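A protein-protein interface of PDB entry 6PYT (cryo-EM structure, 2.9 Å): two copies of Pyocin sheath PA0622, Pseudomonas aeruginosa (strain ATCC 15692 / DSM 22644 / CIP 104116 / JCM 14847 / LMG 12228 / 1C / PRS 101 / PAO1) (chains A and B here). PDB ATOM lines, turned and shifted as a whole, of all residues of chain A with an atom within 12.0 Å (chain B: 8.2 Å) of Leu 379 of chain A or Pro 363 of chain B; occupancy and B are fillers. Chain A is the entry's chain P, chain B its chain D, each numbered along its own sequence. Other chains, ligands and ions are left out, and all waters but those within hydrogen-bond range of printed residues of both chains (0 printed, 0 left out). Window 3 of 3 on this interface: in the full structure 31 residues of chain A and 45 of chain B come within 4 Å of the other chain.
The backbone carbonyl oxygen (O) of Thr 375 of chain A is in hydrogen-bond range of the side-chain hydroxyl (OG1) of Thr 360 of chain B (3.1 Å).
The backbone NH (N) of Trp 378 of chain A lies close to the side-chain hydroxyl (OG1) of Thr 360 of chain B (3.3 Å).
The backbone NH of Ile 332 of chain B lies within hydrogen-bond range of the backbone carbonyl oxygen of Thr 360 of chain B (3.0 Å).
Printed residues of chain B within 4 Å of Val 374 of chain A: Arg 283 (3.4 Å).
Of the printed residues of chain B, Gln 377 of chain A touches Thr 360 (3.8 Å).
Of chain B, only Pro 363 comes within 4 Å of Leu 379 of chain A.
Of the printed residues of chain B, Leu 383 of chain A touches Ile 332 and Pro 363.
Thr 360 of chain B touches just these residues of chain A: Thr 375, Gln 377 and Trp 378.
No residue of chain A comes within 4 Å of Asp 361 of chain B.
No residue of chain A comes within 4 Å of Val 362 of chain B.
Of chain A, only Leu 379 and Leu 383 come within 4 Å of Pro 363 of chain B.
No residue of chain A comes within 4 Å of Pro 364 of chain B.
No residue of chain A comes within 4 Å of Ala 365 of chain B.
The nearest printed residue of chain B that does not touch Gln 377 of chain A is Asn 333 of chain B (6.6 Å).
Of the 14 printed residues of chain A, 7 touch a printed residue of chain B.
Printed residues of chain A that touch a printed residue of chain B: Val 374, Thr 375, Gln 377, Trp 378, Leu 379, Val 382 and Leu 383.
Hydrophobic or aromatic side chains of chain A within 4 Å of the printed part of chain B: Val 374, Trp 378, Leu 379, Val 382 and Leu 383.
Of the 20 printed residues of chain B, 5 touch a printed residue of chain A.
Hydrophobic or aromatic side chains of chain B that line the printed part of chain A: Ile 332 and Pro 363.
Arg 283 of chain B touches Val 374 of chain A.
Gln 377 of chain A touches Thr 360 of chain B (N to OG1, 3.8 Å).
CD1 of Ile 332 of chain B touches O of Trp 378 of chain A, at 3.5 Å.
Asn 333 of chain B touches Trp 378 of chain A.
CG of Pro 363 of chain B touches CD2 of Leu 379 of chain A, at 3.8 Å.
Val 382 of chain A touches Ile 332 of chain B.
Asn 333 of chain B touches Val 382 of chain A (OD1 to CG1, 3.4 Å).
CD1 of Ile 332 of chain B touches CD1 of Leu 383 of chain A (3.9 Å).
Pro 363 of chain B touches Leu 383 of chain A (CD to CD1, 3.9 Å).
No position is printed for both chains.
Of the 11 pairs that touch across the chains among the printed residues, none has its exchanged pair printed and touching as well.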
ATOM      1  N   GLU A 373     -20.101  25.930  27.237  1.00  0.00           N
ATOM      2  CA  GLU A 373     -21.108  25.189  26.494  1.00  0.00           C
ATOM      3  C   GLU A 373     -20.453  24.446  25.342  1.00  0.00           C
ATOM      4  O   GLU A 373     -19.613  25.004  24.637  1.00  0.00           O
ATOM      5  CB  GLU A 373     -22.172  26.128  25.937  1.00  0.00           C
ATOM      6  N   VAL A 374     -20.849  23.197  25.141  1.00  0.00           N
ATOM      7  CA  VAL A 374     -20.428  22.422  23.984  1.00  0.00           C
ATOM      8  C   VAL A 374     -21.536  22.497  22.945  1.00  0.00           C
ATOM      9  O   VAL A 374     -22.672  22.083  23.206  1.00  0.00           O
ATOM     10  CB  VAL A 374     -20.135  20.965  24.357  1.00  0.00           C
ATOM     11  CG1 VAL A 374     -19.675  20.239  23.145  1.00  0.00           C
ATOM     12  CG2 VAL A 374     -19.095  20.892  25.430  1.00  0.00           C
ATOM     13  N   THR A 375     -21.215  23.015  21.768  1.00  0.00           N
ATOM     14  CA  THR A 375     -22.184  23.185  20.699  1.00  0.00           C
ATOM     15  C   THR A 375     -21.806  22.320  19.506  1.00  0.00           C
ATOM     16  O   THR A 375     -20.687  21.815  19.399  1.00  0.00           O
ATOM     17  CB  THR A 375     -22.281  24.652  20.266  1.00  0.00           C
ATOM     18  OG1 THR A 375     -21.012  25.091  19.774  1.00  0.00           O
ATOM     19  CG2 THR A 375     -22.652  25.510  21.429  1.00  0.00           C
ATOM     20  N   ASP A 376     -22.765  22.143  18.605  1.00  0.00           N
ATOM     21  CA  ASP A 376     -22.511  21.591  17.282  1.00  0.00           C
ATOM     22  C   ASP A 376     -22.647  22.664  16.213  1.00  0.00           C
ATOM     23  O   ASP A 376     -23.015  22.372  15.075  1.00  0.00           O
ATOM     24  CB  ASP A 376     -23.452  20.427  16.987  1.00  0.00           C
ATOM     25  N   GLN A 377     -22.373  23.918  16.582  1.00  0.00           N
ATOM     26  CA  GLN A 377     -22.509  25.024  15.644  1.00  0.00           C
ATOM     27  C   GLN A 377     -21.447  24.954  14.560  1.00  0.00           C
ATOM     28  O   GLN A 377     -21.757  25.034  13.366  1.00  0.00           O
ATOM     29  CB  GLN A 377     -22.426  26.354  16.388  1.00  0.00           C
ATOM     30  CG  GLN A 377     -22.538  27.557  15.484  1.00  0.00           C
ATOM     31  CD  GLN A 377     -22.456  28.852  16.247  1.00  0.00           C
ATOM     32  OE1 GLN A 377     -22.310  28.853  17.459  1.00  0.00           O
ATOM     33  NE2 GLN A 377     -22.529  29.964  15.538  1.00  0.00           N
ATOM     34  N   TRP A 378     -20.188  24.793  14.952  1.00  0.00           N
ATOM     35  CA  TRP A 378     -19.102  24.696  13.982  1.00  0.00           C
ATOM     36  C   TRP A 378     -18.797  23.249  13.629  1.00  0.00           C
ATOM     37  O   TRP A 378     -17.647  22.828  13.573  1.00  0.00           O
ATOM     38  CB  TRP A 378     -17.868  25.390  14.528  1.00  0.00           C
ATOM     39  CG  TRP A 378     -18.088  26.821  14.793  1.00  0.00           C
ATOM     40  CD1 TRP A 378     -17.964  27.842  13.911  1.00  0.00           C
ATOM     41  CD2 TRP A 378     -18.460  27.406  16.038  1.00  0.00           C
ATOM     42  NE1 TRP A 378     -18.239  29.033  14.526  1.00  0.00           N
ATOM     43  CE2 TRP A 378     -18.543  28.789  15.838  1.00  0.00           C
ATOM     44  CE3 TRP A 378     -18.725  26.893  17.309  1.00  0.00           C
ATOM     45  CZ2 TRP A 378     -18.883  29.664  16.853  1.00  0.00           C
ATOM     46  CZ3 TRP A 378     -19.056  27.757  18.312  1.00  0.00           C
ATOM     47  CH2 TRP A 378     -19.136  29.127  18.082  1.00  0.00           C
ATOM     48  N   LEU A 379     -19.843  22.481  13.358  1.00  0.00           N
ATOM     49  CA  LEU A 379     -19.691  21.131  12.849  1.00  0.00           C
ATOM     50  C   LEU A 379     -19.820  21.105  11.337  1.00  0.00           C
ATOM     51  O   LEU A 379     -19.338  20.166  10.697  1.00  0.00           O
ATOM     52  CB  LEU A 379     -20.733  20.224  13.519  1.00  0.00           C
ATOM     53  CG  LEU A 379     -20.670  18.699  13.608  1.00  0.00           C
ATOM     54  CD1 LEU A 379     -21.156  17.997  12.359  1.00  0.00           C
ATOM     55  CD2 LEU A 379     -19.263  18.263  13.945  1.00  0.00           C
ATOM     56  N   THR A 380     -20.420  22.144  10.763  1.00  0.00           N
ATOM     57  CA  THR A 380     -20.531  22.324   9.325  1.00  0.00           C
ATOM     58  C   THR A 380     -19.513  23.305   8.772  1.00  0.00           C
ATOM     59  O   THR A 380     -19.083  23.147   7.625  1.00  0.00           O
ATOM     60  CB  THR A 380     -21.923  22.838   8.965  1.00  0.00           C
ATOM     61  OG1 THR A 380     -22.073  24.164   9.483  1.00  0.00           O
ATOM     62  CG2 THR A 380     -22.982  21.962   9.591  1.00  0.00           C
ATOM     63  N   GLU A 381     -19.139  24.317   9.567  1.00  0.00           N
ATOM     64  CA  GLU A 381     -18.174  25.334   9.145  1.00  0.00           C
ATOM     65  C   GLU A 381     -16.816  24.721   8.837  1.00  0.00           C
ATOM     66  O   GLU A 381     -16.087  25.212   7.967  1.00  0.00           O
ATOM     67  CB  GLU A 381     -18.026  26.397  10.236  1.00  0.00           C
ATOM     68  N   VAL A 382     -16.471  23.647   9.536  1.00  0.00           N
ATOM     69  CA  VAL A 382     -15.352  22.798   9.169  1.00  0.00           C
ATOM     70  C   VAL A 382     -15.917  21.409   8.942  1.00  0.00           C
ATOM     71  O   VAL A 382     -17.141  21.227   8.968  1.00  0.00           O
ATOM     72  CB  VAL A 382     -14.265  22.802  10.252  1.00  0.00           C
ATOM     73  CG1 VAL A 382     -13.624  24.163  10.337  1.00  0.00           C
ATOM     74  CG2 VAL A 382     -14.884  22.462  11.578  1.00  0.00           C
ATOM     75  N   LEU A 383     -15.027  20.446   8.675  1.00  0.00           N
ATOM     76  CA  LEU A 383     -15.343  19.020   8.510  1.00  0.00           C
ATOM     77  C   LEU A 383     -16.263  18.786   7.318  1.00  0.00           C
ATOM     78  O   LEU A 383     -17.152  17.936   7.353  1.00  0.00           O
ATOM     79  CB  LEU A 383     -15.957  18.418   9.773  1.00  0.00           C
ATOM     80  CG  LEU A 383     -15.241  18.679  11.087  1.00  0.00           C
ATOM     81  CD1 LEU A 383     -15.971  17.979  12.198  1.00  0.00           C
ATOM     82  CD2 LEU A 383     -13.811  18.260  11.009  1.00  0.00           C
ATOM     83  N   ASP A 384     -16.055  19.545   6.251  1.00  0.00           N
ATOM     84  CA  ASP A 384     -16.947  19.476   5.110  1.00  0.00           C
ATOM     85  C   ASP A 384     -16.145  19.839   3.868  1.00  0.00           C
ATOM     86  O   ASP A 384     -15.023  20.342   3.960  1.00  0.00           O
ATOM     87  CB  ASP A 384     -18.156  20.400   5.326  1.00  0.00           C
ATOM     88  N   VAL A 385     -16.723  19.543   2.700  1.00  0.00           N
ATOM     89  CA  VAL A 385     -16.089  19.898   1.434  1.00  0.00           C
ATOM     90  C   VAL A 385     -16.009  21.414   1.288  1.00  0.00           C
ATOM     91  O   VAL A 385     -14.985  21.954   0.846  1.00  0.00           O
ATOM     92  CB  VAL A 385     -16.856  19.251   0.265  1.00  0.00           C
ATOM     93  CG1 VAL A 385     -16.206  19.591  -1.069  1.00  0.00           C
ATOM     94  CG2 VAL A 385     -16.949  17.745   0.460  1.00  0.00           C
ATOM     95  N   ALA A 386     -17.078  22.112   1.679  1.00  0.00           N
ATOM     96  CA  ALA A 386     -17.183  23.579   1.732  1.00  0.00           C
ATOM     97  C   ALA A 386     -16.875  24.282   0.408  1.00  0.00           C
ATOM     98  O   ALA A 386     -15.735  24.663   0.139  1.00  0.00           O
ATOM     99  CB  ALA A 386     -16.284  24.135   2.844  1.00  0.00           C
ATOM    100  OXT ALA A 386     -17.764  24.494  -0.416  1.00  0.00           O
ATOM    101  N   TRP B 218      -9.030  14.456  23.775  1.00  0.00           N
ATOM    102  CA  TRP B 218     -10.233  14.513  22.963  1.00  0.00           C
ATOM    103  C   TRP B 218     -10.439  13.258  22.134  1.00  0.00           C
ATOM    104  O   TRP B 218     -11.529  13.064  21.596  1.00  0.00           O
ATOM    105  CB  TRP B 218     -10.183  15.728  22.040  1.00  0.00           C
ATOM    106  CG  TRP B 218      -9.029  15.700  21.105  1.00  0.00           C
ATOM    107  CD1 TRP B 218      -9.005  15.187  19.846  1.00  0.00           C
ATOM    108  CD2 TRP B 218      -7.716  16.186  21.364  1.00  0.00           C
ATOM    109  NE1 TRP B 218      -7.760  15.333  19.299  1.00  0.00           N
ATOM    110  CE2 TRP B 218      -6.949  15.944  20.215  1.00  0.00           C
ATOM    111  CE3 TRP B 218      -7.113  16.806  22.458  1.00  0.00           C
ATOM    112  CZ2 TRP B 218      -5.613  16.298  20.130  1.00  0.00           C
ATOM    113  CZ3 TRP B 218      -5.795  17.162  22.369  1.00  0.00           C
ATOM    114  CH2 TRP B 218      -5.057  16.908  21.216  1.00  0.00           C
ATOM    115  N   SER B 219      -9.419  12.422  21.993  1.00  0.00           N
ATOM    116  CA  SER B 219      -9.569  11.209  21.212  1.00  0.00           C
ATOM    117  C   SER B 219     -10.321  10.152  22.006  1.00  0.00           C
ATOM    118  O   SER B 219     -10.327  10.147  23.237  1.00  0.00           O
ATOM    119  CB  SER B 219      -8.210  10.664  20.784  1.00  0.00           C
ATOM    120  OG  SER B 219      -7.572  11.532  19.872  1.00  0.00           O
ATOM    121  N   SER B 220     -10.948   9.274  21.296  1.00  0.00           N
ATOM    122  CA  SER B 220     -11.632   8.235  22.041  1.00  0.00           C
ATOM    123  C   SER B 220     -10.691   7.068  22.296  1.00  0.00           C
ATOM    124  O   SER B 220      -9.787   6.807  21.502  1.00  0.00           O
ATOM    125  CB  SER B 220     -12.859   7.746  21.280  1.00  0.00           C
ATOM    126  OG  SER B 220     -12.483   7.032  20.122  1.00  0.00           O
ATOM    127  N   ASN B 269     -17.595   3.498  23.066  1.00  0.00           N
ATOM    128  CA  ASN B 269     -17.276   4.869  23.452  1.00  0.00           C
ATOM    129  C   ASN B 269     -18.476   5.661  23.943  1.00  0.00           C
ATOM    130  O   ASN B 269     -18.369   6.883  24.085  1.00  0.00           O
ATOM    131  CB  ASN B 269     -16.613   5.642  22.316  1.00  0.00           C
ATOM    132  CG  ASN B 269     -17.344   5.514  21.011  1.00  0.00           C
ATOM    133  OD1 ASN B 269     -18.395   4.883  20.927  1.00  0.00           O
ATOM    134  ND2 ASN B 269     -16.784   6.107  19.972  1.00  0.00           N
ATOM    135  N   PHE B 280     -21.149  10.537  24.077  1.00  0.00           N
ATOM    136  CA  PHE B 280     -19.791  10.047  23.917  1.00  0.00           C
ATOM    137  C   PHE B 280     -18.922  10.479  25.081  1.00  0.00           C
ATOM    138  O   PHE B 280     -19.084  11.572  25.624  1.00  0.00           O
ATOM    139  CB  PHE B 280     -19.177  10.569  22.623  1.00  0.00           C
ATOM    140  CG  PHE B 280     -19.937  10.186  21.397  1.00  0.00           C
ATOM    141  CD1 PHE B 280     -19.881   8.897  20.913  1.00  0.00           C
ATOM    142  CD2 PHE B 280     -20.684  11.124  20.712  1.00  0.00           C
ATOM    143  CE1 PHE B 280     -20.573   8.544  19.781  1.00  0.00           C
ATOM    144  CE2 PHE B 280     -21.379  10.777  19.572  1.00  0.00           C
ATOM    145  CZ  PHE B 280     -21.322   9.481  19.109  1.00  0.00           C
ATOM    146  N   THR B 282     -15.893  11.140  24.548  1.00  0.00           N
ATOM    147  CA  THR B 282     -15.186  12.247  23.925  1.00  0.00           C
ATOM    148  C   THR B 282     -15.790  13.584  24.328  1.00  0.00           C
ATOM    149  O   THR B 282     -15.063  14.497  24.722  1.00  0.00           O
ATOM    150  CB  THR B 282     -15.207  12.064  22.409  1.00  0.00           C
ATOM    151  OG1 THR B 282     -14.355  10.970  22.054  1.00  0.00           O
ATOM    152  CG2 THR B 282     -14.784  13.323  21.678  1.00  0.00           C
ATOM    153  N   ARG B 283     -17.121  13.692  24.298  1.00  0.00           N
ATOM    154  CA  ARG B 283     -17.806  14.906  24.732  1.00  0.00           C
ATOM    155  C   ARG B 283     -17.597  15.175  26.213  1.00  0.00           C
ATOM    156  O   ARG B 283     -17.420  16.325  26.619  1.00  0.00           O
ATOM    157  CB  ARG B 283     -19.295  14.790  24.426  1.00  0.00           C
ATOM    158  CG  ARG B 283     -19.605  14.788  22.957  1.00  0.00           C
ATOM    159  CD  ARG B 283     -19.490  16.177  22.433  1.00  0.00           C
ATOM    160  NE  ARG B 283     -20.531  16.994  23.022  1.00  0.00           N
ATOM    161  CZ  ARG B 283     -21.727  17.175  22.476  1.00  0.00           C
ATOM    162  NH1 ARG B 283     -22.021  16.612  21.315  1.00  0.00           N
ATOM    163  NH2 ARG B 283     -22.625  17.934  23.085  1.00  0.00           N
ATOM    164  N   THR B 286     -13.582  15.899  26.925  1.00  0.00           N
ATOM    165  CA  THR B 286     -13.067  17.138  26.346  1.00  0.00           C
ATOM    166  C   THR B 286     -13.548  18.341  27.132  1.00  0.00           C
ATOM    167  O   THR B 286     -12.750  19.207  27.493  1.00  0.00           O
ATOM    168  CB  THR B 286     -13.487  17.276  24.886  1.00  0.00           C
ATOM    169  OG1 THR B 286     -13.006  16.153  24.145  1.00  0.00           O
ATOM    170  CG2 THR B 286     -12.938  18.545  24.275  1.00  0.00           C
ATOM    171  N   GLY B 329      -6.075  20.484  17.984  1.00  0.00           N
ATOM    172  CA  GLY B 329      -7.199  19.701  17.528  1.00  0.00           C
ATOM    173  C   GLY B 329      -8.194  19.294  18.583  1.00  0.00           C
ATOM    174  O   GLY B 329      -8.996  18.393  18.328  1.00  0.00           O
ATOM    175  N   ALA B 330      -8.177  19.923  19.758  1.00  0.00           N
ATOM    176  CA  ALA B 330      -9.106  19.530  20.810  1.00  0.00           C
ATOM    177  C   ALA B 330     -10.511  20.022  20.510  1.00  0.00           C
ATOM    178  O   ALA B 330     -11.495  19.321  20.768  1.00  0.00           O
ATOM    179  CB  ALA B 330      -8.637  20.068  22.159  1.00  0.00           C
ATOM    180  N   VAL B 331     -10.622  21.234  19.978  1.00  0.00           N
ATOM    181  CA  VAL B 331     -11.893  21.842  19.634  1.00  0.00           C
ATOM    182  C   VAL B 331     -11.853  22.195  18.158  1.00  0.00           C
ATOM    183  O   VAL B 331     -10.866  21.949  17.465  1.00  0.00           O
ATOM    184  CB  VAL B 331     -12.180  23.097  20.479  1.00  0.00           C
ATOM    185  CG1 VAL B 331     -12.172  22.747  21.948  1.00  0.00           C
ATOM    186  CG2 VAL B 331     -11.162  24.175  20.195  1.00  0.00           C
ATOM    187  N   ILE B 332     -12.947  22.783  17.685  1.00  0.00           N
ATOM    188  CA  ILE B 332     -13.030  23.376  16.357  1.00  0.00           C
ATOM    189  C   ILE B 332     -13.846  24.663  16.453  1.00  0.00           C
ATOM    190  O   ILE B 332     -15.060  24.620  16.687  1.00  0.00           O
ATOM    191  CB  ILE B 332     -13.615  22.399  15.323  1.00  0.00           C
ATOM    192  CG1 ILE B 332     -14.727  21.538  15.928  1.00  0.00           C
ATOM    193  CG2 ILE B 332     -12.533  21.552  14.685  1.00  0.00           C
ATOM    194  CD1 ILE B 332     -15.372  20.599  14.963  1.00  0.00           C
ATOM    195  N   ASN B 333     -13.169  25.806  16.302  1.00  0.00           N
ATOM    196  CA  ASN B 333     -13.761  27.151  16.240  1.00  0.00           C
ATOM    197  C   ASN B 333     -14.567  27.481  17.501  1.00  0.00           C
ATOM    198  O   ASN B 333     -15.780  27.605  17.479  1.00  0.00           O
ATOM    199  CB  ASN B 333     -14.618  27.334  14.984  1.00  0.00           C
ATOM    200  CG  ASN B 333     -13.809  27.250  13.710  1.00  0.00           C
ATOM    201  OD1 ASN B 333     -14.002  26.345  12.901  1.00  0.00           O
ATOM    202  ND2 ASN B 333     -12.895  28.194  13.522  1.00  0.00           N
ATOM    203  N   THR B 360     -17.029  23.764  20.116  1.00  0.00           N
ATOM    204  CA  THR B 360     -17.494  22.563  19.432  1.00  0.00           C
ATOM    205  C   THR B 360     -16.444  21.472  19.563  1.00  0.00           C
ATOM    206  O   THR B 360     -15.271  21.696  19.254  1.00  0.00           O
ATOM    207  CB  THR B 360     -17.776  22.828  17.950  1.00  0.00           C
ATOM    208  OG1 THR B 360     -18.829  23.782  17.829  1.00  0.00           O
ATOM    209  CG2 THR B 360     -18.208  21.566  17.246  1.00  0.00           C
ATOM    210  N   ASP B 361     -16.867  20.298  20.012  1.00  0.00           N
ATOM    211  CA  ASP B 361     -15.973  19.168  20.189  1.00  0.00           C
ATOM    212  C   ASP B 361     -15.849  18.381  18.891  1.00  0.00           C
ATOM    213  O   ASP B 361     -16.740  18.406  18.041  1.00  0.00           O
ATOM    214  CB  ASP B 361     -16.492  18.262  21.300  1.00  0.00           C
ATOM    215  N   VAL B 362     -14.732  17.681  18.745  1.00  0.00           N
ATOM    216  CA  VAL B 362     -14.506  16.851  17.560  1.00  0.00           C
ATOM    217  C   VAL B 362     -15.307  15.558  17.697  1.00  0.00           C
ATOM    218  O   VAL B 362     -15.280  14.926  18.764  1.00  0.00           O
ATOM    219  CB  VAL B 362     -13.016  16.577  17.367  1.00  0.00           C
ATOM    220  CG1 VAL B 362     -12.338  17.817  16.865  1.00  0.00           C
ATOM    221  CG2 VAL B 362     -12.351  16.209  18.678  1.00  0.00           C
ATOM    222  N   PRO B 363     -16.057  15.156  16.675  1.00  0.00           N
ATOM    223  CA  PRO B 363     -16.868  13.948  16.781  1.00  0.00           C
ATOM    224  C   PRO B 363     -16.047  12.708  16.481  1.00  0.00           C
ATOM    225  O   PRO B 363     -15.201  12.716  15.577  1.00  0.00           O
ATOM    226  CB  PRO B 363     -17.955  14.166  15.722  1.00  0.00           C
ATOM    227  CG  PRO B 363     -17.314  15.046  14.722  1.00  0.00           C
ATOM    228  CD  PRO B 363     -16.384  15.939  15.475  1.00  0.00           C
ATOM    229  N   PRO B 364     -16.254  11.625  17.223  1.00  0.00           N
ATOM    230  CA  PRO B 364     -15.568  10.373  16.902  1.00  0.00           C
ATOM    231  C   PRO B 364     -16.245   9.641  15.755  1.00  0.00           C
ATOM    232  O   PRO B 364     -17.466   9.654  15.605  1.00  0.00           O
ATOM    233  CB  PRO B 364     -15.673   9.574  18.205  1.00  0.00           C
ATOM    234  CG  PRO B 364     -16.902  10.080  18.841  1.00  0.00           C
ATOM    235  CD  PRO B 364     -16.994  11.535  18.490  1.00  0.00           C
ATOM    236  N   ALA B 365     -15.422   8.991  14.934  1.00  0.00           N
ATOM    237  CA  ALA B 365     -15.904   8.272  13.755  1.00  0.00           C
ATOM    238  C   ALA B 365     -16.474   6.931  14.201  1.00  0.00           C
ATOM    239  O   ALA B 365     -15.867   5.874  14.032  1.00  0.00           O
ATOM    240  CB  ALA B 365     -14.781   8.094  12.743  1.00  0.00           C
ATOM    241  N   GLU B 366     -17.685   6.986  14.752  1.00  0.00           N
ATOM    242  CA  GLU B 366     -18.247   5.838  15.458  1.00  0.00           C
ATOM    243  C   GLU B 366     -18.670   4.738  14.497  1.00  0.00           C
ATOM    244  O   GLU B 366     -18.517   3.551  14.799  1.00  0.00           O
ATOM    245  CB  GLU B 366     -19.445   6.279  16.297  1.00  0.00           C
